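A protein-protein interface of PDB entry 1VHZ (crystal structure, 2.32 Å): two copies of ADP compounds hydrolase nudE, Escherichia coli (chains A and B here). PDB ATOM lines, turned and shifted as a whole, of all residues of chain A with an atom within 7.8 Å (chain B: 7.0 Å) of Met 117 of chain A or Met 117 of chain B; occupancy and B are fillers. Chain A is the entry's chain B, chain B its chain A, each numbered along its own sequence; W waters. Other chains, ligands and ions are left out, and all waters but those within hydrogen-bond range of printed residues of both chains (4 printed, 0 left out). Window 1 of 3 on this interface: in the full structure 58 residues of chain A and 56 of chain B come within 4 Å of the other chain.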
ATOM      1  N   THR A  72     -18.293  -9.641 -28.807  1.00  0.00           N
ATOM      2  CA  THR A  72     -18.744  -8.938 -30.008  1.00  0.00           C
ATOM      3  C   THR A  72     -19.264  -9.945 -31.030  1.00  0.00           C
ATOM      4  O   THR A  72     -19.621  -9.538 -32.128  1.00  0.00           O
ATOM      5  CB  THR A  72     -17.575  -8.149 -30.657  1.00  0.00           C
ATOM      6  OG1 THR A  72     -16.463  -9.041 -30.825  1.00  0.00           O
ATOM      7  CG2 THR A  72     -17.152  -6.999 -29.771  1.00  0.00           C
ATOM      8  N   GLU A  76     -11.562 -11.804 -33.911  1.00  0.00           N
ATOM      9  CA  GLU A  76     -10.574 -10.746 -33.778  1.00  0.00           C
ATOM     10  C   GLU A  76      -9.358 -11.119 -34.658  1.00  0.00           C
ATOM     11  O   GLU A  76      -9.167 -12.285 -34.993  1.00  0.00           O
ATOM     12  CB  GLU A  76     -10.013 -10.690 -32.366  1.00  0.00           C
ATOM     13  CG  GLU A  76     -10.841 -10.138 -31.229  1.00  0.00           C
ATOM     14  CD  GLU A  76      -9.938  -9.906 -30.008  1.00  0.00           C
ATOM     15  OE1 GLU A  76     -10.018 -10.713 -29.059  1.00  0.00           O
ATOM     16  OE2 GLU A  76      -9.128  -8.955 -30.025  1.00  0.00           O
ATOM     17  N   LEU A 115       0.786  -3.016 -18.837  1.00  0.00           N
ATOM     18  CA  LEU A 115      -0.335  -2.089 -18.894  1.00  0.00           C
ATOM     19  C   LEU A 115      -1.536  -2.532 -18.061  1.00  0.00           C
ATOM     20  O   LEU A 115      -1.826  -3.717 -17.894  1.00  0.00           O
ATOM     21  CB  LEU A 115      -0.781  -2.003 -20.344  1.00  0.00           C
ATOM     22  CG  LEU A 115      -0.385  -0.911 -21.301  1.00  0.00           C
ATOM     23  CD1 LEU A 115       0.906  -0.186 -21.020  1.00  0.00           C
ATOM     24  CD2 LEU A 115      -0.362  -1.474 -22.726  1.00  0.00           C
ATOM     25  N   SER A 116      -2.253  -1.548 -17.542  1.00  0.00           N
ATOM     26  CA  SER A 116      -3.488  -1.766 -16.793  1.00  0.00           C
ATOM     27  C   SER A 116      -4.607  -1.732 -17.836  1.00  0.00           C
ATOM     28  O   SER A 116      -4.360  -1.228 -18.951  1.00  0.00           O
ATOM     29  CB  SER A 116      -3.733  -0.547 -15.845  1.00  0.00           C
ATOM     30  OG  SER A 116      -2.675  -0.565 -14.889  1.00  0.00           O
ATOM     31  N   MET A 117      -5.804  -2.146 -17.480  1.00  0.00           N
ATOM     32  CA  MET A 117      -6.935  -2.091 -18.422  1.00  0.00           C
ATOM     33  C   MET A 117      -8.169  -1.621 -17.647  1.00  0.00           C
ATOM     34  O   MET A 117      -8.665  -2.357 -16.805  1.00  0.00           O
ATOM     35  CB  MET A 117      -7.177  -3.462 -19.033  1.00  0.00           C
ATOM     36  CG  MET A 117      -7.182  -3.554 -20.537  1.00  0.00           C
ATOM     37  SD  MET A 117      -8.215  -2.350 -21.382  1.00  0.00           S
ATOM     38  CE  MET A 117      -8.741  -3.298 -22.808  1.00  0.00           C
ATOM     39  N   ALA A 118      -8.648  -0.418 -17.898  1.00  0.00           N
ATOM     40  CA  ALA A 118      -9.807   0.104 -17.185  1.00  0.00           C
ATOM     41  C   ALA A 118      -9.745  -0.185 -15.686  1.00  0.00           C
ATOM     42  O   ALA A 118     -10.600  -0.874 -15.114  1.00  0.00           O
ATOM     43  CB  ALA A 118     -11.088  -0.435 -17.809  1.00  0.00           C
ATOM     44  N   PRO A 119      -8.781   0.431 -14.994  1.00  0.00           N
ATOM     45  CA  PRO A 119      -8.589   0.308 -13.566  1.00  0.00           C
ATOM     46  C   PRO A 119      -9.774   0.768 -12.736  1.00  0.00           C
ATOM     47  O   PRO A 119      -9.825   0.541 -11.526  1.00  0.00           O
ATOM     48  CB  PRO A 119      -7.366   1.160 -13.252  1.00  0.00           C
ATOM     49  CG  PRO A 119      -7.217   2.071 -14.417  1.00  0.00           C
ATOM     50  CD  PRO A 119      -7.740   1.300 -15.607  1.00  0.00           C
ATOM     51  N   SER A 120     -10.718   1.505 -13.302  1.00  0.00           N
ATOM     52  CA  SER A 120     -11.912   1.939 -12.597  1.00  0.00           C
ATOM     53  C   SER A 120     -12.735   0.733 -12.146  1.00  0.00           C
ATOM     54  O   SER A 120     -13.447   0.805 -11.144  1.00  0.00           O
ATOM     55  CB  SER A 120     -12.787   2.812 -13.514  1.00  0.00           C
ATOM     56  OG  SER A 120     -12.350   4.159 -13.459  1.00  0.00           O
ATOM     57  N   TYR A 121     -12.730  -0.358 -12.916  1.00  0.00           N
ATOM     58  CA  TYR A 121     -13.497  -1.533 -12.531  1.00  0.00           C
ATOM     59  C   TYR A 121     -12.655  -2.789 -12.392  1.00  0.00           C
ATOM     60  O   TYR A 121     -13.108  -3.761 -11.791  1.00  0.00           O
ATOM     61  CB  TYR A 121     -14.621  -1.832 -13.534  1.00  0.00           C
ATOM     62  CG  TYR A 121     -15.492  -0.646 -13.867  1.00  0.00           C
ATOM     63  CD1 TYR A 121     -16.359  -0.098 -12.937  1.00  0.00           C
ATOM     64  CD2 TYR A 121     -15.419  -0.063 -15.125  1.00  0.00           C
ATOM     65  CE1 TYR A 121     -17.146   0.994 -13.251  1.00  0.00           C
ATOM     66  CE2 TYR A 121     -16.201   1.032 -15.451  1.00  0.00           C
ATOM     67  CZ  TYR A 121     -17.061   1.554 -14.510  1.00  0.00           C
ATOM     68  OH  TYR A 121     -17.836   2.648 -14.832  1.00  0.00           O
ATOM     69  N   PHE A 122     -11.503  -2.834 -13.048  1.00  0.00           N
ATOM     70  CA  PHE A 122     -10.657  -4.035 -13.011  1.00  0.00           C
ATOM     71  C   PHE A 122      -9.275  -3.705 -12.482  1.00  0.00           C
ATOM     72  O   PHE A 122      -8.893  -2.531 -12.465  1.00  0.00           O
ATOM     73  CB  PHE A 122     -10.558  -4.654 -14.422  1.00  0.00           C
ATOM     74  CG  PHE A 122     -11.882  -4.652 -15.144  1.00  0.00           C
ATOM     75  CD1 PHE A 122     -12.226  -3.601 -15.976  1.00  0.00           C
ATOM     76  CD2 PHE A 122     -12.813  -5.653 -14.925  1.00  0.00           C
ATOM     77  CE1 PHE A 122     -13.459  -3.568 -16.609  1.00  0.00           C
ATOM     78  CE2 PHE A 122     -14.043  -5.627 -15.555  1.00  0.00           C
ATOM     79  CZ  PHE A 122     -14.371  -4.582 -16.399  1.00  0.00           C
ATOM     80  N   SER A 123      -8.521  -4.689 -12.022  1.00  0.00           N
ATOM     81  CA  SER A 123      -7.180  -4.418 -11.511  1.00  0.00           C
ATOM     82  C   SER A 123      -6.138  -5.259 -12.248  1.00  0.00           C
ATOM     83  O   SER A 123      -4.943  -5.223 -11.913  1.00  0.00           O
ATOM     84  CB  SER A 123      -7.129  -4.694 -10.009  1.00  0.00           C
ATOM     85  OG  SER A 123      -7.214  -6.091  -9.774  1.00  0.00           O
ATOM     86  N   SER A 124      -6.556  -5.988 -13.270  1.00  0.00           N
ATOM     87  CA  SER A 124      -5.650  -6.827 -14.035  1.00  0.00           C
ATOM     88  C   SER A 124      -4.595  -6.093 -14.852  1.00  0.00           C
ATOM     89  O   SER A 124      -4.814  -5.041 -15.458  1.00  0.00           O
ATOM     90  CB  SER A 124      -6.490  -7.709 -14.997  1.00  0.00           C
ATOM     91  OG  SER A 124      -5.791  -8.945 -15.148  1.00  0.00           O
ATOM     92  N   LYS A 125      -3.424  -6.705 -14.976  1.00  0.00           N
ATOM     93  CA  LYS A 125      -2.309  -6.158 -15.734  1.00  0.00           C
ATOM     94  C   LYS A 125      -2.036  -7.000 -16.982  1.00  0.00           C
ATOM     95  O   LYS A 125      -2.246  -8.202 -16.956  1.00  0.00           O
ATOM     96  CB  LYS A 125      -1.019  -6.174 -14.910  1.00  0.00           C
ATOM     97  CG  LYS A 125      -1.136  -5.605 -13.516  1.00  0.00           C
ATOM     98  CD  LYS A 125      -1.319  -4.102 -13.525  1.00  0.00           C
ATOM     99  CE  LYS A 125      -1.057  -3.535 -12.124  1.00  0.00           C
ATOM    100  NZ  LYS A 125      -1.421  -2.094 -12.060  1.00  0.00           N
ATOM    101  N   MET A 126      -1.526  -6.368 -18.026  1.00  0.00           N
ATOM    102  CA  MET A 126      -1.192  -7.039 -19.265  1.00  0.00           C
ATOM    103  C   MET A 126       0.271  -6.765 -19.614  1.00  0.00           C
ATOM    104  O   MET A 126       0.680  -5.609 -19.727  1.00  0.00           O
ATOM    105  CB  MET A 126      -2.105  -6.601 -20.400  1.00  0.00           C
ATOM    106  CG  MET A 126      -1.631  -7.019 -21.788  1.00  0.00           C
ATOM    107  SD  MET A 126      -1.619  -8.802 -21.986  1.00  0.00           S
ATOM    108  CE  MET A 126      -3.376  -9.126 -22.240  1.00  0.00           C
ATOM    109  N   ASN A 167      -8.544  -3.496 -34.288  1.00  0.00           N
ATOM    110  CA  ASN A 167      -8.594  -2.293 -33.471  1.00  0.00           C
ATOM    111  C   ASN A 167      -9.161  -2.390 -32.084  1.00  0.00           C
ATOM    112  O   ASN A 167     -10.230  -1.870 -31.773  1.00  0.00           O
ATOM    113  CB  ASN A 167      -9.223  -1.142 -34.296  1.00  0.00           C
ATOM    114  CG  ASN A 167      -8.327  -0.742 -35.461  1.00  0.00           C
ATOM    115  OD1 ASN A 167      -7.103  -0.872 -35.415  1.00  0.00           O
ATOM    116  ND2 ASN A 167      -8.859  -0.248 -36.581  1.00  0.00           N
ATOM    117  N   GLU A 168      -8.399  -2.981 -31.184  1.00  0.00           N
ATOM    118  CA  GLU A 168      -8.674  -3.217 -29.777  1.00  0.00           C
ATOM    119  C   GLU A 168      -7.536  -2.569 -28.983  1.00  0.00           C
ATOM    120  O   GLU A 168      -6.367  -2.610 -29.394  1.00  0.00           O
ATOM    121  CB  GLU A 168      -8.823  -4.714 -29.535  1.00  0.00           C
ATOM    122  CG  GLU A 168      -9.241  -5.074 -28.118  1.00  0.00           C
ATOM    123  CD  GLU A 168      -8.074  -5.223 -27.158  1.00  0.00           C
ATOM    124  OE1 GLU A 168      -6.903  -5.262 -27.593  1.00  0.00           O
ATOM    125  OE2 GLU A 168      -8.343  -5.322 -25.945  1.00  0.00           O
ATOM    126  N   ALA A 169      -7.834  -1.925 -27.876  1.00  0.00           N
ATOM    127  CA  ALA A 169      -6.831  -1.153 -27.140  1.00  0.00           C
ATOM    128  C   ALA A 169      -5.525  -1.836 -26.845  1.00  0.00           C
ATOM    129  O   ALA A 169      -4.491  -1.148 -26.916  1.00  0.00           O
ATOM    130  CB  ALA A 169      -7.446  -0.520 -25.898  1.00  0.00           C
ATOM    131  N   ARG A 170      -5.515  -3.105 -26.457  1.00  0.00           N
ATOM    132  CA  ARG A 170      -4.272  -3.818 -26.170  1.00  0.00           C
ATOM    133  C   ARG A 170      -3.481  -4.111 -27.426  1.00  0.00           C
ATOM    134  O   ARG A 170      -2.251  -3.909 -27.419  1.00  0.00           O
ATOM    135  CB  ARG A 170      -4.561  -5.064 -25.327  1.00  0.00           C
ATOM    136  CG  ARG A 170      -5.163  -4.632 -23.960  1.00  0.00           C
ATOM    137  CD  ARG A 170      -5.746  -5.844 -23.243  1.00  0.00           C
ATOM    138  NE  ARG A 170      -6.582  -6.639 -24.088  1.00  0.00           N
ATOM    139  CZ  ARG A 170      -7.121  -7.823 -23.883  1.00  0.00           C
ATOM    140  NH1 ARG A 170      -6.921  -8.467 -22.743  1.00  0.00           N
ATOM    141  NH2 ARG A 170      -7.865  -8.386 -24.835  1.00  0.00           N
ATOM    142  N   ASN A 171      -4.133  -4.568 -28.508  1.00  0.00           N
ATOM    143  CA  ASN A 171      -3.409  -4.798 -29.755  1.00  0.00           C
ATOM    144  C   ASN A 171      -2.782  -3.487 -30.260  1.00  0.00           C
ATOM    145  O   ASN A 171      -1.642  -3.483 -30.703  1.00  0.00           O
ATOM    146  CB  ASN A 171      -4.339  -5.292 -30.892  1.00  0.00           C
ATOM    147  CG  ASN A 171      -4.828  -6.707 -30.671  1.00  0.00           C
ATOM    148  OD1 ASN A 171      -4.204  -7.496 -29.972  1.00  0.00           O
ATOM    149  ND2 ASN A 171      -5.959  -7.076 -31.265  1.00  0.00           N
ATOM    150  N   ALA B  51     -18.525   4.801 -25.567  1.00  0.00           N
ATOM    151  CA  ALA B  51     -17.758   5.728 -24.785  1.00  0.00           C
ATOM    152  C   ALA B  51     -16.973   6.685 -25.674  1.00  0.00           C
ATOM    153  O   ALA B  51     -16.771   6.461 -26.871  1.00  0.00           O
ATOM    154  CB  ALA B  51     -16.791   4.982 -23.850  1.00  0.00           C
ATOM    155  N   LEU B 115     -12.199   2.306 -30.865  1.00  0.00           N
ATOM    156  CA  LEU B 115     -11.550   1.069 -30.424  1.00  0.00           C
ATOM    157  C   LEU B 115     -12.447   0.188 -29.569  1.00  0.00           C
ATOM    158  O   LEU B 115     -13.229   0.699 -28.788  1.00  0.00           O
ATOM    159  CB  LEU B 115     -10.352   1.458 -29.551  1.00  0.00           C
ATOM    160  CG  LEU B 115      -8.938   1.484 -30.052  1.00  0.00           C
ATOM    161  CD1 LEU B 115      -8.760   1.681 -31.543  1.00  0.00           C
ATOM    162  CD2 LEU B 115      -8.133   2.545 -29.287  1.00  0.00           C
ATOM    163  N   SER B 116     -12.226  -1.115 -29.687  1.00  0.00           N
ATOM    164  CA  SER B 116     -12.919  -2.079 -28.828  1.00  0.00           C
ATOM    165  C   SER B 116     -11.965  -2.389 -27.666  1.00  0.00           C
ATOM    166  O   SER B 116     -10.781  -1.993 -27.746  1.00  0.00           O
ATOM    167  CB  SER B 116     -13.143  -3.361 -29.648  1.00  0.00           C
ATOM    168  OG  SER B 116     -11.924  -4.086 -29.680  1.00  0.00           O
ATOM    169  N   MET B 117     -12.423  -2.957 -26.568  1.00  0.00           N
ATOM    170  CA  MET B 117     -11.552  -3.303 -25.443  1.00  0.00           C
ATOM    171  C   MET B 117     -11.930  -4.701 -24.929  1.00  0.00           C
ATOM    172  O   MET B 117     -13.027  -4.937 -24.445  1.00  0.00           O
ATOM    173  CB  MET B 117     -11.641  -2.314 -24.296  1.00  0.00           C
ATOM    174  CG  MET B 117     -11.567  -0.829 -24.541  1.00  0.00           C
ATOM    175  SD  MET B 117     -13.162  -0.064 -24.883  1.00  0.00           S
ATOM    176  CE  MET B 117     -13.349   1.045 -23.491  1.00  0.00           C
ATOM    177  N   ALA B 118     -11.040  -5.671 -25.064  1.00  0.00           N
ATOM    178  CA  ALA B 118     -11.305  -7.042 -24.639  1.00  0.00           C
ATOM    179  C   ALA B 118     -12.684  -7.523 -25.072  1.00  0.00           C
ATOM    180  O   ALA B 118     -13.574  -7.813 -24.268  1.00  0.00           O
ATOM    181  CB  ALA B 118     -11.095  -7.185 -23.136  1.00  0.00           C
ATOM    182  N   PRO B 119     -12.891  -7.663 -26.386  1.00  0.00           N
ATOM    183  CA  PRO B 119     -14.125  -8.124 -26.979  1.00  0.00           C
ATOM    184  C   PRO B 119     -14.505  -9.550 -26.654  1.00  0.00           C
ATOM    185  O   PRO B 119     -15.607 -10.023 -26.971  1.00  0.00           O
ATOM    186  CB  PRO B 119     -13.940  -7.911 -28.477  1.00  0.00           C
ATOM    187  CG  PRO B 119     -12.465  -7.889 -28.682  1.00  0.00           C
ATOM    188  CD  PRO B 119     -11.883  -7.310 -27.420  1.00  0.00           C
ATOM    189  N   SER B 120     -13.640 -10.330 -26.014  1.00  0.00           N
ATOM    190  CA  SER B 120     -13.981 -11.696 -25.625  1.00  0.00           C
ATOM    191  C   SER B 120     -15.042 -11.678 -24.526  1.00  0.00           C
ATOM    192  O   SER B 120     -15.856 -12.589 -24.438  1.00  0.00           O
ATOM    193  CB  SER B 120     -12.742 -12.441 -25.110  1.00  0.00           C
ATOM    194  OG  SER B 120     -12.017 -12.995 -26.197  1.00  0.00           O
ATOM    195  N   TYR B 121     -15.014 -10.669 -23.666  1.00  0.00           N
ATOM    196  CA  TYR B 121     -15.933 -10.503 -22.567  1.00  0.00           C
ATOM    197  C   TYR B 121     -16.809  -9.270 -22.637  1.00  0.00           C
ATOM    198  O   TYR B 121     -17.861  -9.230 -21.989  1.00  0.00           O
ATOM    199  CB  TYR B 121     -15.136 -10.431 -21.230  1.00  0.00           C
ATOM    200  CG  TYR B 121     -14.198 -11.618 -21.115  1.00  0.00           C
ATOM    201  CD1 TYR B 121     -14.666 -12.863 -20.731  1.00  0.00           C
ATOM    202  CD2 TYR B 121     -12.865 -11.489 -21.481  1.00  0.00           C
ATOM    203  CE1 TYR B 121     -13.814 -13.950 -20.669  1.00  0.00           C
ATOM    204  CE2 TYR B 121     -12.008 -12.573 -21.428  1.00  0.00           C
ATOM    205  CZ  TYR B 121     -12.491 -13.799 -21.023  1.00  0.00           C
ATOM    206  OH  TYR B 121     -11.633 -14.873 -20.967  1.00  0.00           O
ATOM    207  N   PHE B 122     -16.383  -8.215 -23.329  1.00  0.00           N
ATOM    208  CA  PHE B 122     -17.161  -6.981 -23.406  1.00  0.00           C
ATOM    209  C   PHE B 122     -17.339  -6.533 -24.851  1.00  0.00           C
ATOM    210  O   PHE B 122     -16.440  -6.751 -25.674  1.00  0.00           O
ATOM    211  CB  PHE B 122     -16.476  -5.833 -22.641  1.00  0.00           C
ATOM    212  CG  PHE B 122     -15.894  -6.228 -21.314  1.00  0.00           C
ATOM    213  CD1 PHE B 122     -14.565  -6.615 -21.220  1.00  0.00           C
ATOM    214  CD2 PHE B 122     -16.673  -6.249 -20.171  1.00  0.00           C
ATOM    215  CE1 PHE B 122     -14.020  -7.003 -20.006  1.00  0.00           C
ATOM    216  CE2 PHE B 122     -16.135  -6.637 -18.959  1.00  0.00           C
ATOM    217  CZ  PHE B 122     -14.810  -7.020 -18.877  1.00  0.00           C
ATOM    218  N   SER B 123     -18.416  -5.830 -25.151  1.00  0.00           N
ATOM    219  CA  SER B 123     -18.638  -5.352 -26.512  1.00  0.00           C
ATOM    220  C   SER B 123     -18.523  -3.833 -26.613  1.00  0.00           C
ATOM    221  O   SER B 123     -18.830  -3.257 -27.671  1.00  0.00           O
ATOM    222  CB  SER B 123     -20.046  -5.779 -26.963  1.00  0.00           C
ATOM    223  OG  SER B 123     -21.001  -5.199 -26.075  1.00  0.00           O
ATOM    224  N   SER B 124     -18.068  -3.161 -25.573  1.00  0.00           N
ATOM    225  CA  SER B 124     -17.963  -1.711 -25.585  1.00  0.00           C
ATOM    226  C   SER B 124     -16.916  -1.122 -26.517  1.00  0.00           C
ATOM    227  O   SER B 124     -15.830  -1.649 -26.682  1.00  0.00           O
ATOM    228  CB  SER B 124     -17.688  -1.196 -24.153  1.00  0.00           C
ATOM    229  OG  SER B 124     -18.264   0.101 -24.041  1.00  0.00           O
ATOM    230  N   LYS B 125     -17.218   0.032 -27.099  1.00  0.00           N
ATOM    231  CA  LYS B 125     -16.350   0.749 -27.993  1.00  0.00           C
ATOM    232  C   LYS B 125     -15.968   2.104 -27.364  1.00  0.00           C
ATOM    233  O   LYS B 125     -16.808   2.747 -26.738  1.00  0.00           O
ATOM    234  CB  LYS B 125     -16.978   1.108 -29.339  1.00  0.00           C
ATOM    235  CG  LYS B 125     -17.765   0.045 -30.048  1.00  0.00           C
ATOM    236  CD  LYS B 125     -16.876  -1.028 -30.645  1.00  0.00           C
ATOM    237  CE  LYS B 125     -17.735  -2.019 -31.440  1.00  0.00           C
ATOM    238  NZ  LYS B 125     -17.131  -3.377 -31.364  1.00  0.00           N
ATOM    239  N   MET B 126     -14.764   2.526 -27.718  1.00  0.00           N
ATOM    240  CA  MET B 126     -14.248   3.803 -27.235  1.00  0.00           C
ATOM    241  C   MET B 126     -13.883   4.700 -28.407  1.00  0.00           C
ATOM    242  O   MET B 126     -13.091   4.336 -29.282  1.00  0.00           O
ATOM    243  CB  MET B 126     -13.082   3.535 -26.301  1.00  0.00           C
ATOM    244  CG  MET B 126     -12.228   4.749 -25.946  1.00  0.00           C
ATOM    245  SD  MET B 126     -13.147   5.944 -24.978  1.00  0.00           S
ATOM    246  CE  MET B 126     -13.069   5.208 -23.349  1.00  0.00           C
ATOM    247  N   ASN B 167      -0.131   4.447 -17.642  1.00  0.00           N
ATOM    248  CA  ASN B 167      -0.016   3.271 -18.493  1.00  0.00           C
ATOM    249  C   ASN B 167      -1.180   2.310 -18.514  1.00  0.00           C
ATOM    250  O   ASN B 167      -1.128   1.196 -18.005  1.00  0.00           O
ATOM    251  CB  ASN B 167       1.331   2.563 -18.235  1.00  0.00           C
ATOM    252  CG  ASN B 167       2.477   3.434 -18.751  1.00  0.00           C
ATOM    253  OD1 ASN B 167       2.293   4.301 -19.605  1.00  0.00           O
ATOM    254  ND2 ASN B 167       3.677   3.262 -18.238  1.00  0.00           N
ATOM    255  N   GLU B 168      -2.263   2.729 -19.143  1.00  0.00           N
ATOM    256  CA  GLU B 168      -3.515   2.005 -19.320  1.00  0.00           C
ATOM    257  C   GLU B 168      -3.731   1.890 -20.828  1.00  0.00           C
ATOM    258  O   GLU B 168      -3.481   2.863 -21.549  1.00  0.00           O
ATOM    259  CB  GLU B 168      -4.630   2.724 -18.579  1.00  0.00           C
ATOM    260  CG  GLU B 168      -5.968   2.016 -18.580  1.00  0.00           C
ATOM    261  CD  GLU B 168      -6.782   2.288 -19.829  1.00  0.00           C
ATOM    262  OE1 GLU B 168      -6.490   3.284 -20.529  1.00  0.00           O
ATOM    263  OE2 GLU B 168      -7.722   1.524 -20.106  1.00  0.00           O
ATOM    264  N   ALA B 169      -4.170   0.737 -21.325  1.00  0.00           N
ATOM    265  CA  ALA B 169      -4.292   0.506 -22.755  1.00  0.00           C
ATOM    266  C   ALA B 169      -4.997   1.560 -23.575  1.00  0.00           C
ATOM    267  O   ALA B 169      -4.553   1.796 -24.728  1.00  0.00           O
ATOM    268  CB  ALA B 169      -4.874  -0.876 -23.079  1.00  0.00           C
ATOM    269  N   ARG B 170      -6.080   2.136 -23.109  1.00  0.00           N
ATOM    270  CA  ARG B 170      -6.805   3.165 -23.866  1.00  0.00           C
ATOM    271  C   ARG B 170      -6.019   4.470 -23.872  1.00  0.00           C
ATOM    272  O   ARG B 170      -5.954   5.113 -24.927  1.00  0.00           O
ATOM    273  CB  ARG B 170      -8.211   3.348 -23.289  1.00  0.00           C
ATOM    274  CG  ARG B 170      -9.066   2.085 -23.509  1.00  0.00           C
ATOM    275  CD  ARG B 170     -10.338   2.115 -22.641  1.00  0.00           C
ATOM    276  NE  ARG B 170     -10.039   2.493 -21.280  1.00  0.00           N
ATOM    277  CZ  ARG B 170     -10.898   2.828 -20.334  1.00  0.00           C
ATOM    278  NH1 ARG B 170     -10.480   3.178 -19.114  1.00  0.00           N
ATOM    279  NH2 ARG B 170     -12.191   2.835 -20.597  1.00  0.00           N
HETATM  280  O   HOH W   1     -10.725 -13.327 -28.916  1.00  0.00           O
HETATM  281  O   HOH W   2     -10.509   3.436 -15.807  1.00  0.00           O
HETATM  282  O   HOH W   3     -10.276 -10.264 -26.441  1.00  0.00           O
HETATM  283  O   HOH W   4       0.032   1.020 -15.315  1.00  0.00           O
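N of Ser 116 of chain B is in hydrogen-bond range of O of Asn 167 of chain A (3.0 Å). The backbone NH (N) of Ala 169 of chain A lies within hydrogen-bond range of the backbone carbonyl oxygen (O) of Ser 116 of chain B, at 3.0 Å. The backbone NH (N) of Ala 118 of chain B lies within hydrogen-bond range of the side-chain carboxylate (OE2) of Glu 168 of chain A. O of Pro 119 of chain B is in hydrogen-bond range of N of Thr 72 of chain A (3.3 Å). O of Asn 167 of chain B lies within hydrogen-bond range of N of Ser 116 of chain A, 3.0 Å away. N of Ala 118 of chain A lies within hydrogen-bond range of OE2 of Glu 168 of chain B (3.1 Å). N of Ala 169 of chain B sits at hydrogen-bond distance from O of Ser 116 of chain A (3.1 Å).
N of Ala 51 of chain B lies within hydrogen-bond range of O of Lys 125 of chain B, at 2.9 Å. The backbone carbonyl oxygen of Leu 115 of chain B lies within hydrogen-bond range of the backbone NH of Met 126 of chain B (2.6 Å). The backbone carbonyl oxygen (O) of Leu 115 of chain A sits at hydrogen-bond distance from the backbone NH (N) of Met 126 of chain A (2.7 Å). The side-chain hydroxyl (OG) of Ser 116 of chain A is in hydrogen-bond range of the side-chain amino group (NZ) of Lys 125 of chain A (3.5 Å). The guanidinium group (NE) of Arg 170 of chain A is in salt-bridge range of the side-chain carboxylate (OE2) of Glu 168 of chain A (2.9 Å). OE1 of Glu 168 of chain A sits at hydrogen-bond distance from N of Asn 171 of chain A (3.0 Å).
CG2 of Thr 72 of chain A touches NZ of Lys 125 of chain B, 3.96 Å away. CD of Glu 76 of chain A touches CG of Pro 119 of chain B (3.5 Å). Leu 115 of chain A touches Asn 167 of chain B (CA to O, 3.5 Å). CA of Glu 168 of chain B touches O of Ser 116 of chain A, 3.4 Å away. Pro 119 of chain A touches Glu 168 of chain B (CD to CG, 3.5 Å). Leu 115 of chain B touches Asn 167 of chain A. OE2 of Glu 168 of chain A touches C of Met 117 of chain B (3.8 Å). CB of Ala 169 of chain A touches CG of Arg 170 of chain B, 3.9 Å away. Arg 170 of chain A touches Ala 118 of chain B (NH2 to CA, 3.7 Å). CB of Ala 169 of chain B touches CG of Arg 170 of chain A (3.9 Å).
Of the printed residues of chain B, Met 117 of chain A touches Met 117 (3.4 Å). Printed residues of chain A within 4 Å of Met 117 of chain B: Met 117 (3.4 Å) and Glu 168 (3.8 Å). Of the printed residues of chain A, Ser 123 of chain B touches Thr 72. Printed residues of chain B within 4 Å of Ala 169 of chain A: Ser 116, Ala 169 and Arg 170. Of the printed residues of chain A, Phe 122 of chain B touches Phe 122. Of the printed residues of chain A, Glu 168 of chain B touches Ser 116, Ala 118 and Pro 119. Asn 171 of chain A touches none of the printed residues of chain B. The nearest printed residue of chain A that does not touch Met 117 of chain B is Ala 169 of chain A (4.3 Å).
Printed residues of chain B that touch a printed residue of chain A: Leu 115, Ser 116, Met 117, Ala 118, Pro 119, Phe 122, Ser 123, Lys 125, Asn 167, Glu 168, Ala 169 and Arg 170. Hydrophobic or aromatic side chains of chain B that line the printed part of chain A: Leu 115, Met 117, Ala 118, Pro 119, Phe 122 and Ala 169. Along chain B the printed residues that touch a printed residue of chain A span positions 115 to 170.
Ser 116 of chain A touches Asn 167 of chain B, and with the chains exchanged Asn 167 of chain A touches Ser 116 of chain B. Met 117 of chain B touches its own counterpart, Met 117 of chain A. Glu 168 of chain A touches Met 117 of chain B, but with the chains exchanged Met 117 of chain A does not touch Glu 168 of chain B (4.02 Å). Ala 169 of chain A touches Arg 170 of chain B, and with the chains exchanged Arg 170 of chain A touches Ala 169 of chain B. Of the 24 pairs that touch across the chains among the printed residues, 19 have their exchanged pair printed and touching as well.
Water W3 lies within hydrogen-bond range of the side-chain carboxylate of Glu 76 of chain A (2.7 Å), the side-chain hydroxyl of Ser 120 of chain B (3.2 Å) and the guanidinium group of Arg 170 of chain A (3.5 Å). Water W1 bridges the side-chain carboxylate of Glu 76 of chain A (2.7 Å) and the side-chain hydroxyl of Ser 120 of chain B (3.0 Å). Water W4 bridges O of Asn 167 of chain B (2.9 Å) and OG of Ser 116 of chain A (3.2 Å). Water W2 lies within hydrogen-bond range of OG of Ser 120 of chain A and NH1 of Arg 170 of chain B.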
